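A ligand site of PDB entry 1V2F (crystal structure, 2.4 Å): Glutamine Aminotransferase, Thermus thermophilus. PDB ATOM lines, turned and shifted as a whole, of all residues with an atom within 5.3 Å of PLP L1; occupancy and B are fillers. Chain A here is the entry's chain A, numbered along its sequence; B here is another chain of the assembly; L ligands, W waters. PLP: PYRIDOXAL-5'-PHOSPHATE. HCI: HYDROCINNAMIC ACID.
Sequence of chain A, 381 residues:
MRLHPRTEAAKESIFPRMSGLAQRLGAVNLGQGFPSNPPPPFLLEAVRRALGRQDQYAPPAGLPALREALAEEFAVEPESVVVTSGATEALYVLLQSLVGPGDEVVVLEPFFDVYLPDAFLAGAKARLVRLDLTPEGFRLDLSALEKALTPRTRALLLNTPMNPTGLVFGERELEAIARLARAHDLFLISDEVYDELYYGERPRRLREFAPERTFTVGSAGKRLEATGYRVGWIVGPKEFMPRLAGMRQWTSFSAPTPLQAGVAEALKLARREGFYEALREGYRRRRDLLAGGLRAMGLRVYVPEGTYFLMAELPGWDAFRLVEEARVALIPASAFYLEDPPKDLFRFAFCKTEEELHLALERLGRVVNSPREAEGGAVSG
N of Ala 87 lies within hydrogen-bond range of O1P of PLP L1 (2.8 Å). O3P of PLP L1 lies within hydrogen-bond range of N of Thr 88, 2.8 Å away. The side-chain hydroxyl (OG) of Ser 219 sits at hydrogen-bond distance from an oxygen (O1P) of PLP L1 (2.6 Å). O3 of PLP L1 lies close to OH of Tyr 194 (3.5 Å). NZ of Lys 222 is covalently linked to C4A of PLP L1 (1.4 Å). NH2 of Arg 230 lies within salt-bridge range of O3P of PLP L1, 2.8 Å away. O2P of PLP L1 sits at hydrogen-bond distance from OH of Tyr 57 of chain B. The side-chain amide nitrogen (ND2) of Asn 163 lies within hydrogen-bond range of an oxygen (O3) of PLP L1 (3.2 Å). An oxygen (O3P) of PLP L1 sits at hydrogen-bond distance from the side-chain hydroxyl (OG1) of Thr 88 (2.8 Å). ND2 of Asn 163 is in hydrogen-bond range of O1 of HCI L2, at 2.8 Å. The side-chain carboxylate (OD2) of Asp 191 sits at hydrogen-bond distance from a nitrogen (N1) of PLP L1 (2.6 Å).
The backbone NH of Asn 163 sits at hydrogen-bond distance from the side-chain amide oxygen of Asn 159, 2.9 Å away. The side-chain amino group (NZ) of Lys 222 sits at hydrogen-bond distance from the side-chain hydroxyl (OH) of Tyr 194 (3.3 Å). The backbone carbonyl oxygen (O) of Thr 227 sits at hydrogen-bond distance from the guanidinium group (NH1) of Arg 230 (3.0 Å). The side-chain hydroxyl (OH) of Tyr 115 is in hydrogen-bond range of the side-chain carboxylate (OD2) of Asp 191 (2.7 Å). The side-chain hydroxyl (OG) of Ser 219 lies close to the backbone NH (N) of Gly 221 (3.3 Å). The backbone NH of Val 193 sits close to the side-chain carboxylate of Asp 191 (3.5 Å). N of Lys 222 sits at hydrogen-bond distance from OG of Ser 219 (3.3 Å). The backbone NH (N) of Tyr 57 of chain B is in hydrogen-bond range of the side-chain hydroxyl (OG1) of Thr 227.
Gly 86 touches PLP L1 (CA to O1P, 3.4 Å). Leu 91 touches PLP L1. CE1 of Phe 112 touches N1 of PLP L1, at 3.5 Å. Asn 159 touches PLP L1. CG2 of Val 193 touches C3 of PLP L1 (3.5 Å). Hydrophobic or aromatic side chains that line PLP L1: Ala 87, Leu 91, Phe 112, Val 193, Tyr 194 and Tyr 57 of chain B. The nearest printed residue that does not touch PLP L1 is Tyr 115 (4.1 Å).
Water W1 lies within hydrogen-bond range of O2P of PLP L1, O of Thr 227 and OG of Ser 219. Water W2 lies within hydrogen-bond range of O1P of PLP L1, O of Val 231, OG of Ser 219 and N of Gly 221.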
ATOM      1  N   SER A  85       6.713  24.829  14.566  1.00  0.00           N
ATOM      2  CA  SER A  85       6.023  24.965  13.301  1.00  0.00           C
ATOM      3  C   SER A  85       6.949  24.470  12.195  1.00  0.00           C
ATOM      4  O   SER A  85       7.479  25.246  11.401  1.00  0.00           O
ATOM      5  CB  SER A  85       5.654  26.429  13.093  1.00  0.00           C
ATOM      6  OG  SER A  85       4.828  26.893  14.162  1.00  0.00           O
ATOM      7  N   GLY A  86       7.130  23.146  12.163  1.00  0.00           N
ATOM      8  CA  GLY A  86       8.004  22.533  11.173  1.00  0.00           C
ATOM      9  C   GLY A  86       9.423  22.394  11.706  1.00  0.00           C
ATOM     10  O   GLY A  86       9.823  23.110  12.623  1.00  0.00           O
ATOM     11  N   ALA A  87      10.185  21.451  11.155  1.00  0.00           N
ATOM     12  CA  ALA A  87      11.563  21.278  11.578  1.00  0.00           C
ATOM     13  C   ALA A  87      12.330  22.552  11.221  1.00  0.00           C
ATOM     14  O   ALA A  87      13.353  22.869  11.824  1.00  0.00           O
ATOM     15  CB  ALA A  87      12.201  20.073  10.883  1.00  0.00           C
ATOM     16  N   THR A  88      11.829  23.292  10.233  1.00  0.00           N
ATOM     17  CA  THR A  88      12.471  24.535   9.810  1.00  0.00           C
ATOM     18  C   THR A  88      12.588  25.477  10.994  1.00  0.00           C
ATOM     19  O   THR A  88      13.648  26.057  11.229  1.00  0.00           O
ATOM     20  CB  THR A  88      11.698  25.230   8.652  1.00  0.00           C
ATOM     21  OG1 THR A  88      11.874  24.480   7.453  1.00  0.00           O
ATOM     22  CG2 THR A  88      12.235  26.635   8.418  1.00  0.00           C
ATOM     23  N   GLU A  89      11.497  25.647  11.745  1.00  0.00           N
ATOM     24  CA  GLU A  89      11.506  26.514  12.902  1.00  0.00           C
ATOM     25  C   GLU A  89      12.369  25.919  14.022  1.00  0.00           C
ATOM     26  O   GLU A  89      13.079  26.635  14.714  1.00  0.00           O
ATOM     27  CB  GLU A  89      10.091  26.761  13.429  1.00  0.00           C
ATOM     28  CG  GLU A  89      10.062  27.765  14.562  1.00  0.00           C
ATOM     29  CD  GLU A  89       8.672  28.009  15.120  1.00  0.00           C
ATOM     30  OE1 GLU A  89       8.068  27.055  15.649  1.00  0.00           O
ATOM     31  OE2 GLU A  89       8.194  29.162  15.040  1.00  0.00           O
ATOM     32  N   LEU A  91      15.033  24.175  13.775  1.00  0.00           N
ATOM     33  CA  LEU A  91      16.410  24.477  13.420  1.00  0.00           C
ATOM     34  C   LEU A  91      16.759  25.944  13.645  1.00  0.00           C
ATOM     35  O   LEU A  91      17.840  26.258  14.150  1.00  0.00           O
ATOM     36  CB  LEU A  91      16.666  24.097  11.948  1.00  0.00           C
ATOM     37  CG  LEU A  91      16.754  22.585  11.673  1.00  0.00           C
ATOM     38  CD1 LEU A  91      16.743  22.313  10.185  1.00  0.00           C
ATOM     39  CD2 LEU A  91      18.030  22.055  12.308  1.00  0.00           C
ATOM     40  N   PHE A 112      22.067  21.277   4.052  1.00  0.00           N
ATOM     41  CA  PHE A 112      20.653  21.517   3.817  1.00  0.00           C
ATOM     42  C   PHE A 112      20.474  23.043   3.723  1.00  0.00           C
ATOM     43  O   PHE A 112      21.182  23.797   4.371  1.00  0.00           O
ATOM     44  CB  PHE A 112      19.803  20.918   4.963  1.00  0.00           C
ATOM     45  CG  PHE A 112      18.328  21.169   4.820  1.00  0.00           C
ATOM     46  CD1 PHE A 112      17.654  21.969   5.737  1.00  0.00           C
ATOM     47  CD2 PHE A 112      17.632  20.693   3.708  1.00  0.00           C
ATOM     48  CE1 PHE A 112      16.311  22.288   5.550  1.00  0.00           C
ATOM     49  CE2 PHE A 112      16.292  21.008   3.513  1.00  0.00           C
ATOM     50  CZ  PHE A 112      15.624  21.817   4.437  1.00  0.00           C
ATOM     51  N   TYR A 115      20.704  25.687   7.009  1.00  0.00           N
ATOM     52  CA  TYR A 115      21.793  25.727   7.983  1.00  0.00           C
ATOM     53  C   TYR A 115      22.619  27.020   8.015  1.00  0.00           C
ATOM     54  O   TYR A 115      22.664  27.690   9.052  1.00  0.00           O
ATOM     55  CB  TYR A 115      22.713  24.511   7.803  1.00  0.00           C
ATOM     56  CG  TYR A 115      22.027  23.174   7.995  1.00  0.00           C
ATOM     57  CD1 TYR A 115      20.792  23.077   8.634  1.00  0.00           C
ATOM     58  CD2 TYR A 115      22.607  21.997   7.513  1.00  0.00           C
ATOM     59  CE1 TYR A 115      20.148  21.842   8.797  1.00  0.00           C
ATOM     60  CE2 TYR A 115      21.977  20.759   7.658  1.00  0.00           C
ATOM     61  CZ  TYR A 115      20.747  20.692   8.295  1.00  0.00           C
ATOM     62  OH  TYR A 115      20.109  19.482   8.388  1.00  0.00           O
ATOM     63  N   ASN A 159      23.043  15.787  10.151  1.00  0.00           N
ATOM     64  CA  ASN A 159      21.805  15.470   9.429  1.00  0.00           C
ATOM     65  C   ASN A 159      21.829  14.013   8.956  1.00  0.00           C
ATOM     66  O   ASN A 159      22.608  13.656   8.085  1.00  0.00           O
ATOM     67  CB  ASN A 159      21.641  16.395   8.221  1.00  0.00           C
ATOM     68  CG  ASN A 159      20.411  16.056   7.362  1.00  0.00           C
ATOM     69  OD1 ASN A 159      20.390  16.332   6.158  1.00  0.00           O
ATOM     70  ND2 ASN A 159      19.394  15.471   7.989  1.00  0.00           N
ATOM     71  N   ASN A 163      20.364  14.775   3.750  1.00  0.00           N
ATOM     72  CA  ASN A 163      19.853  15.445   2.552  1.00  0.00           C
ATOM     73  C   ASN A 163      21.011  16.367   2.162  1.00  0.00           C
ATOM     74  O   ASN A 163      21.406  17.218   2.962  1.00  0.00           O
ATOM     75  CB  ASN A 163      18.611  16.260   2.928  1.00  0.00           C
ATOM     76  CG  ASN A 163      18.082  17.075   1.777  1.00  0.00           C
ATOM     77  OD1 ASN A 163      18.640  17.064   0.677  1.00  0.00           O
ATOM     78  ND2 ASN A 163      16.978  17.793   2.022  1.00  0.00           N
ATOM     79  N   ASP A 191      19.532  16.726  12.765  1.00  0.00           N
ATOM     80  CA  ASP A 191      18.358  16.887  11.919  1.00  0.00           C
ATOM     81  C   ASP A 191      18.000  15.497  11.419  1.00  0.00           C
ATOM     82  O   ASP A 191      18.658  14.953  10.529  1.00  0.00           O
ATOM     83  CB  ASP A 191      18.711  17.796  10.728  1.00  0.00           C
ATOM     84  CG  ASP A 191      17.515  18.125   9.847  1.00  0.00           C
ATOM     85  OD1 ASP A 191      16.523  17.350   9.825  1.00  0.00           O
ATOM     86  OD2 ASP A 191      17.567  19.167   9.162  1.00  0.00           O
ATOM     87  N   VAL A 193      14.751  14.410  10.174  1.00  0.00           N
ATOM     88  CA  VAL A 193      13.396  14.425   9.642  1.00  0.00           C
ATOM     89  C   VAL A 193      13.082  13.157   8.860  1.00  0.00           C
ATOM     90  O   VAL A 193      11.918  12.771   8.762  1.00  0.00           O
ATOM     91  CB  VAL A 193      13.141  15.666   8.733  1.00  0.00           C
ATOM     92  CG1 VAL A 193      13.278  16.938   9.544  1.00  0.00           C
ATOM     93  CG2 VAL A 193      14.104  15.662   7.547  1.00  0.00           C
ATOM     94  N   TYR A 194      14.110  12.526   8.294  1.00  0.00           N
ATOM     95  CA  TYR A 194      13.955  11.288   7.530  1.00  0.00           C
ATOM     96  C   TYR A 194      14.283  10.077   8.375  1.00  0.00           C
ATOM     97  O   TYR A 194      14.674   9.032   7.840  1.00  0.00           O
ATOM     98  CB  TYR A 194      14.873  11.295   6.302  1.00  0.00           C
ATOM     99  CG  TYR A 194      14.454  12.279   5.235  1.00  0.00           C
ATOM    100  CD1 TYR A 194      13.308  12.057   4.467  1.00  0.00           C
ATOM    101  CD2 TYR A 194      15.151  13.466   5.054  1.00  0.00           C
ATOM    102  CE1 TYR A 194      12.877  12.993   3.538  1.00  0.00           C
ATOM    103  CE2 TYR A 194      14.724  14.413   4.120  1.00  0.00           C
ATOM    104  CZ  TYR A 194      13.581  14.169   3.376  1.00  0.00           C
ATOM    105  OH  TYR A 194      13.116  15.123   2.485  1.00  0.00           O
ATOM    106  N   GLY A 218      12.692  16.488  14.354  1.00  0.00           N
ATOM    107  CA  GLY A 218      11.811  15.662  13.543  1.00  0.00           C
ATOM    108  C   GLY A 218      10.775  16.503  12.816  1.00  0.00           C
ATOM    109  O   GLY A 218      10.616  17.693  13.109  1.00  0.00           O
ATOM    110  N   SER A 219      10.078  15.887  11.879  1.00  0.00           N
ATOM    111  CA  SER A 219       9.058  16.584  11.091  1.00  0.00           C
ATOM    112  C   SER A 219       7.880  15.675  10.748  1.00  0.00           C
ATOM    113  O   SER A 219       8.074  14.588  10.215  1.00  0.00           O
ATOM    114  CB  SER A 219       9.675  17.115   9.786  1.00  0.00           C
ATOM    115  OG  SER A 219       8.694  17.669   8.932  1.00  0.00           O
ATOM    116  N   ALA A 220       6.675  16.138  11.037  1.00  0.00           N
ATOM    117  CA  ALA A 220       5.482  15.369  10.712  1.00  0.00           C
ATOM    118  C   ALA A 220       5.299  15.335   9.192  1.00  0.00           C
ATOM    119  O   ALA A 220       4.854  14.330   8.632  1.00  0.00           O
ATOM    120  CB  ALA A 220       4.263  15.990  11.379  1.00  0.00           C
ATOM    121  N   GLY A 221       5.674  16.427   8.539  1.00  0.00           N
ATOM    122  CA  GLY A 221       5.553  16.527   7.095  1.00  0.00           C
ATOM    123  C   GLY A 221       6.438  15.546   6.356  1.00  0.00           C
ATOM    124  O   GLY A 221       6.058  15.058   5.293  1.00  0.00           O
ATOM    125  N   LYS A 222       7.608  15.260   6.906  1.00  0.00           N
ATOM    126  CA  LYS A 222       8.520  14.318   6.258  1.00  0.00           C
ATOM    127  C   LYS A 222       8.249  12.896   6.739  1.00  0.00           C
ATOM    128  O   LYS A 222       8.747  11.941   6.154  1.00  0.00           O
ATOM    129  CB  LYS A 222       9.979  14.710   6.528  1.00  0.00           C
ATOM    130  CG  LYS A 222      10.405  16.044   5.881  1.00  0.00           C
ATOM    131  CD  LYS A 222      10.359  15.979   4.347  1.00  0.00           C
ATOM    132  CE  LYS A 222      10.787  17.309   3.691  1.00  0.00           C
ATOM    133  NZ  LYS A 222      12.075  17.691   4.301  1.00  0.00           N
ATOM    134  N   THR A 227       4.089  17.735   3.830  1.00  0.00           N
ATOM    135  CA  THR A 227       5.054  18.813   4.059  1.00  0.00           C
ATOM    136  C   THR A 227       4.493  20.179   4.380  1.00  0.00           C
ATOM    137  O   THR A 227       5.201  21.006   4.956  1.00  0.00           O
ATOM    138  CB  THR A 227       6.033  18.972   2.875  1.00  0.00           C
ATOM    139  OG1 THR A 227       5.319  19.381   1.707  1.00  0.00           O
ATOM    140  CG2 THR A 227       6.763  17.658   2.610  1.00  0.00           C
ATOM    141  N   ARG A 230       3.293  21.953   8.601  1.00  0.00           N
ATOM    142  CA  ARG A 230       4.117  22.762   9.498  1.00  0.00           C
ATOM    143  C   ARG A 230       4.041  22.336  10.971  1.00  0.00           C
ATOM    144  O   ARG A 230       3.686  23.129  11.843  1.00  0.00           O
ATOM    145  CB  ARG A 230       3.734  24.255   9.385  1.00  0.00           C
ATOM    146  CG  ARG A 230       3.448  24.755   7.956  1.00  0.00           C
ATOM    147  CD  ARG A 230       4.505  24.302   6.947  1.00  0.00           C
ATOM    148  NE  ARG A 230       5.843  24.763   7.310  1.00  0.00           N
ATOM    149  CZ  ARG A 230       6.934  23.998   7.225  1.00  0.00           C
ATOM    150  NH1 ARG A 230       6.829  22.753   6.780  1.00  0.00           N
ATOM    151  NH2 ARG A 230       8.121  24.475   7.572  1.00  0.00           N
ATOM    152  N   VAL A 231       4.345  21.073  11.210  1.00  0.00           N
ATOM    153  CA  VAL A 231       4.367  20.518  12.546  1.00  0.00           C
ATOM    154  C   VAL A 231       5.689  19.788  12.636  1.00  0.00           C
ATOM    155  O   VAL A 231       5.972  18.924  11.828  1.00  0.00           O
ATOM    156  CB  VAL A 231       3.201  19.525  12.784  1.00  0.00           C
ATOM    157  CG1 VAL A 231       3.425  18.754  14.080  1.00  0.00           C
ATOM    158  CG2 VAL A 231       1.883  20.275  12.858  1.00  0.00           C
ATOM    159  N   GLY A 232       6.512  20.164  13.605  1.00  0.00           N
ATOM    160  CA  GLY A 232       7.795  19.522  13.778  1.00  0.00           C
ATOM    161  C   GLY A 232       8.107  19.458  15.257  1.00  0.00           C
ATOM    162  O   GLY A 232       7.295  19.885  16.083  1.00  0.00           O
ATOM    163  N   PHE A 309      15.998  11.280  -1.863  1.00  0.00           N
ATOM    164  CA  PHE A 309      16.850  12.002  -2.793  1.00  0.00           C
ATOM    165  C   PHE A 309      18.022  11.127  -3.228  1.00  0.00           C
ATOM    166  O   PHE A 309      18.437  10.225  -2.494  1.00  0.00           O
ATOM    167  CB  PHE A 309      17.447  13.261  -2.147  1.00  0.00           C
ATOM    168  CG  PHE A 309      16.440  14.271  -1.689  1.00  0.00           C
ATOM    169  CD1 PHE A 309      15.681  14.978  -2.605  1.00  0.00           C
ATOM    170  CD2 PHE A 309      16.261  14.521  -0.337  1.00  0.00           C
ATOM    171  CE1 PHE A 309      14.755  15.930  -2.187  1.00  0.00           C
ATOM    172  CE2 PHE A 309      15.340  15.467   0.109  1.00  0.00           C
ATOM    173  CZ  PHE A 309      14.578  16.176  -0.821  1.00  0.00           C
ATOM    174  N   TYR B  57       4.091  21.733   0.599  1.00  0.00           N
ATOM    175  CA  TYR B  57       4.654  23.076   0.706  1.00  0.00           C
ATOM    176  C   TYR B  57       4.033  24.111  -0.201  1.00  0.00           C
ATOM    177  O   TYR B  57       3.863  23.884  -1.398  1.00  0.00           O
ATOM    178  CB  TYR B  57       6.153  23.086   0.372  1.00  0.00           C
ATOM    179  CG  TYR B  57       7.070  22.413   1.351  1.00  0.00           C
ATOM    180  CD1 TYR B  57       7.157  22.858   2.678  1.00  0.00           C
ATOM    181  CD2 TYR B  57       7.873  21.355   0.952  1.00  0.00           C
ATOM    182  CE1 TYR B  57       8.034  22.264   3.570  1.00  0.00           C
ATOM    183  CE2 TYR B  57       8.753  20.757   1.835  1.00  0.00           C
ATOM    184  CZ  TYR B  57       8.825  21.207   3.144  1.00  0.00           C
ATOM    185  OH  TYR B  57       9.658  20.568   4.011  1.00  0.00           O
HETATM  186  N1  PLP L   1      15.706  19.402   7.375  1.00  0.00           N
HETATM  187  C2  PLP L   1      15.797  18.567   6.311  1.00  0.00           C
HETATM  188  C2A PLP L   1      17.122  17.798   6.086  1.00  0.00           C
HETATM  189  C3  PLP L   1      14.714  18.429   5.448  1.00  0.00           C
HETATM  190  O3  PLP L   1      14.811  17.563   4.332  1.00  0.00           O
HETATM  191  C4  PLP L   1      13.551  19.147   5.688  1.00  0.00           C
HETATM  192  C4A PLP L   1      12.342  18.960   4.732  1.00  0.00           C
HETATM  193  C5  PLP L   1      13.493  20.007   6.818  1.00  0.00           C
HETATM  194  C6  PLP L   1      14.586  20.127   7.646  1.00  0.00           C
HETATM  195  C5A PLP L   1      12.300  20.894   7.170  1.00  0.00           C
HETATM  196  O4P PLP L   1      11.118  20.222   7.587  1.00  0.00           O
HETATM  197  P   PLP L   1       9.802  21.038   7.871  1.00  0.00           P
HETATM  198  O1P PLP L   1       9.083  20.218   8.855  1.00  0.00           O
HETATM  199  O2P PLP L   1       9.190  21.019   6.431  1.00  0.00           O
HETATM  200  O3P PLP L   1      10.036  22.471   8.232  1.00  0.00           O
HETATM  201  C1  HCI L   2      14.401  19.887   0.084  1.00  0.00           C
HETATM  202  O1  HCI L   2      15.580  19.609   0.341  1.00  0.00           O
HETATM  203  O2  HCI L   2      13.965  19.903  -1.093  1.00  0.00           O
HETATM  204  C2  HCI L   2      13.383  19.634   1.189  1.00  0.00           C
HETATM  205  C3  HCI L   2      12.309  20.714   1.255  1.00  0.00           C
HETATM  206  C1' HCI L   2      12.825  22.058   1.742  1.00  0.00           C
HETATM  207  C2' HCI L   2      13.678  22.824   0.952  1.00  0.00           C
HETATM  208  C3' HCI L   2      14.131  24.077   1.387  1.00  0.00           C
HETATM  209  C4' HCI L   2      13.725  24.573   2.629  1.00  0.00           C
HETATM  210  C5' HCI L   2      12.886  23.822   3.427  1.00  0.00           C
HETATM  211  C6' HCI L   2      12.436  22.564   2.984  1.00  0.00           C
HETATM  212  O   HOH W   1       7.231  19.084   6.360  1.00  0.00           O
HETATM  213  O   HOH W   2       6.109  19.660   8.749  1.00  0.00           O
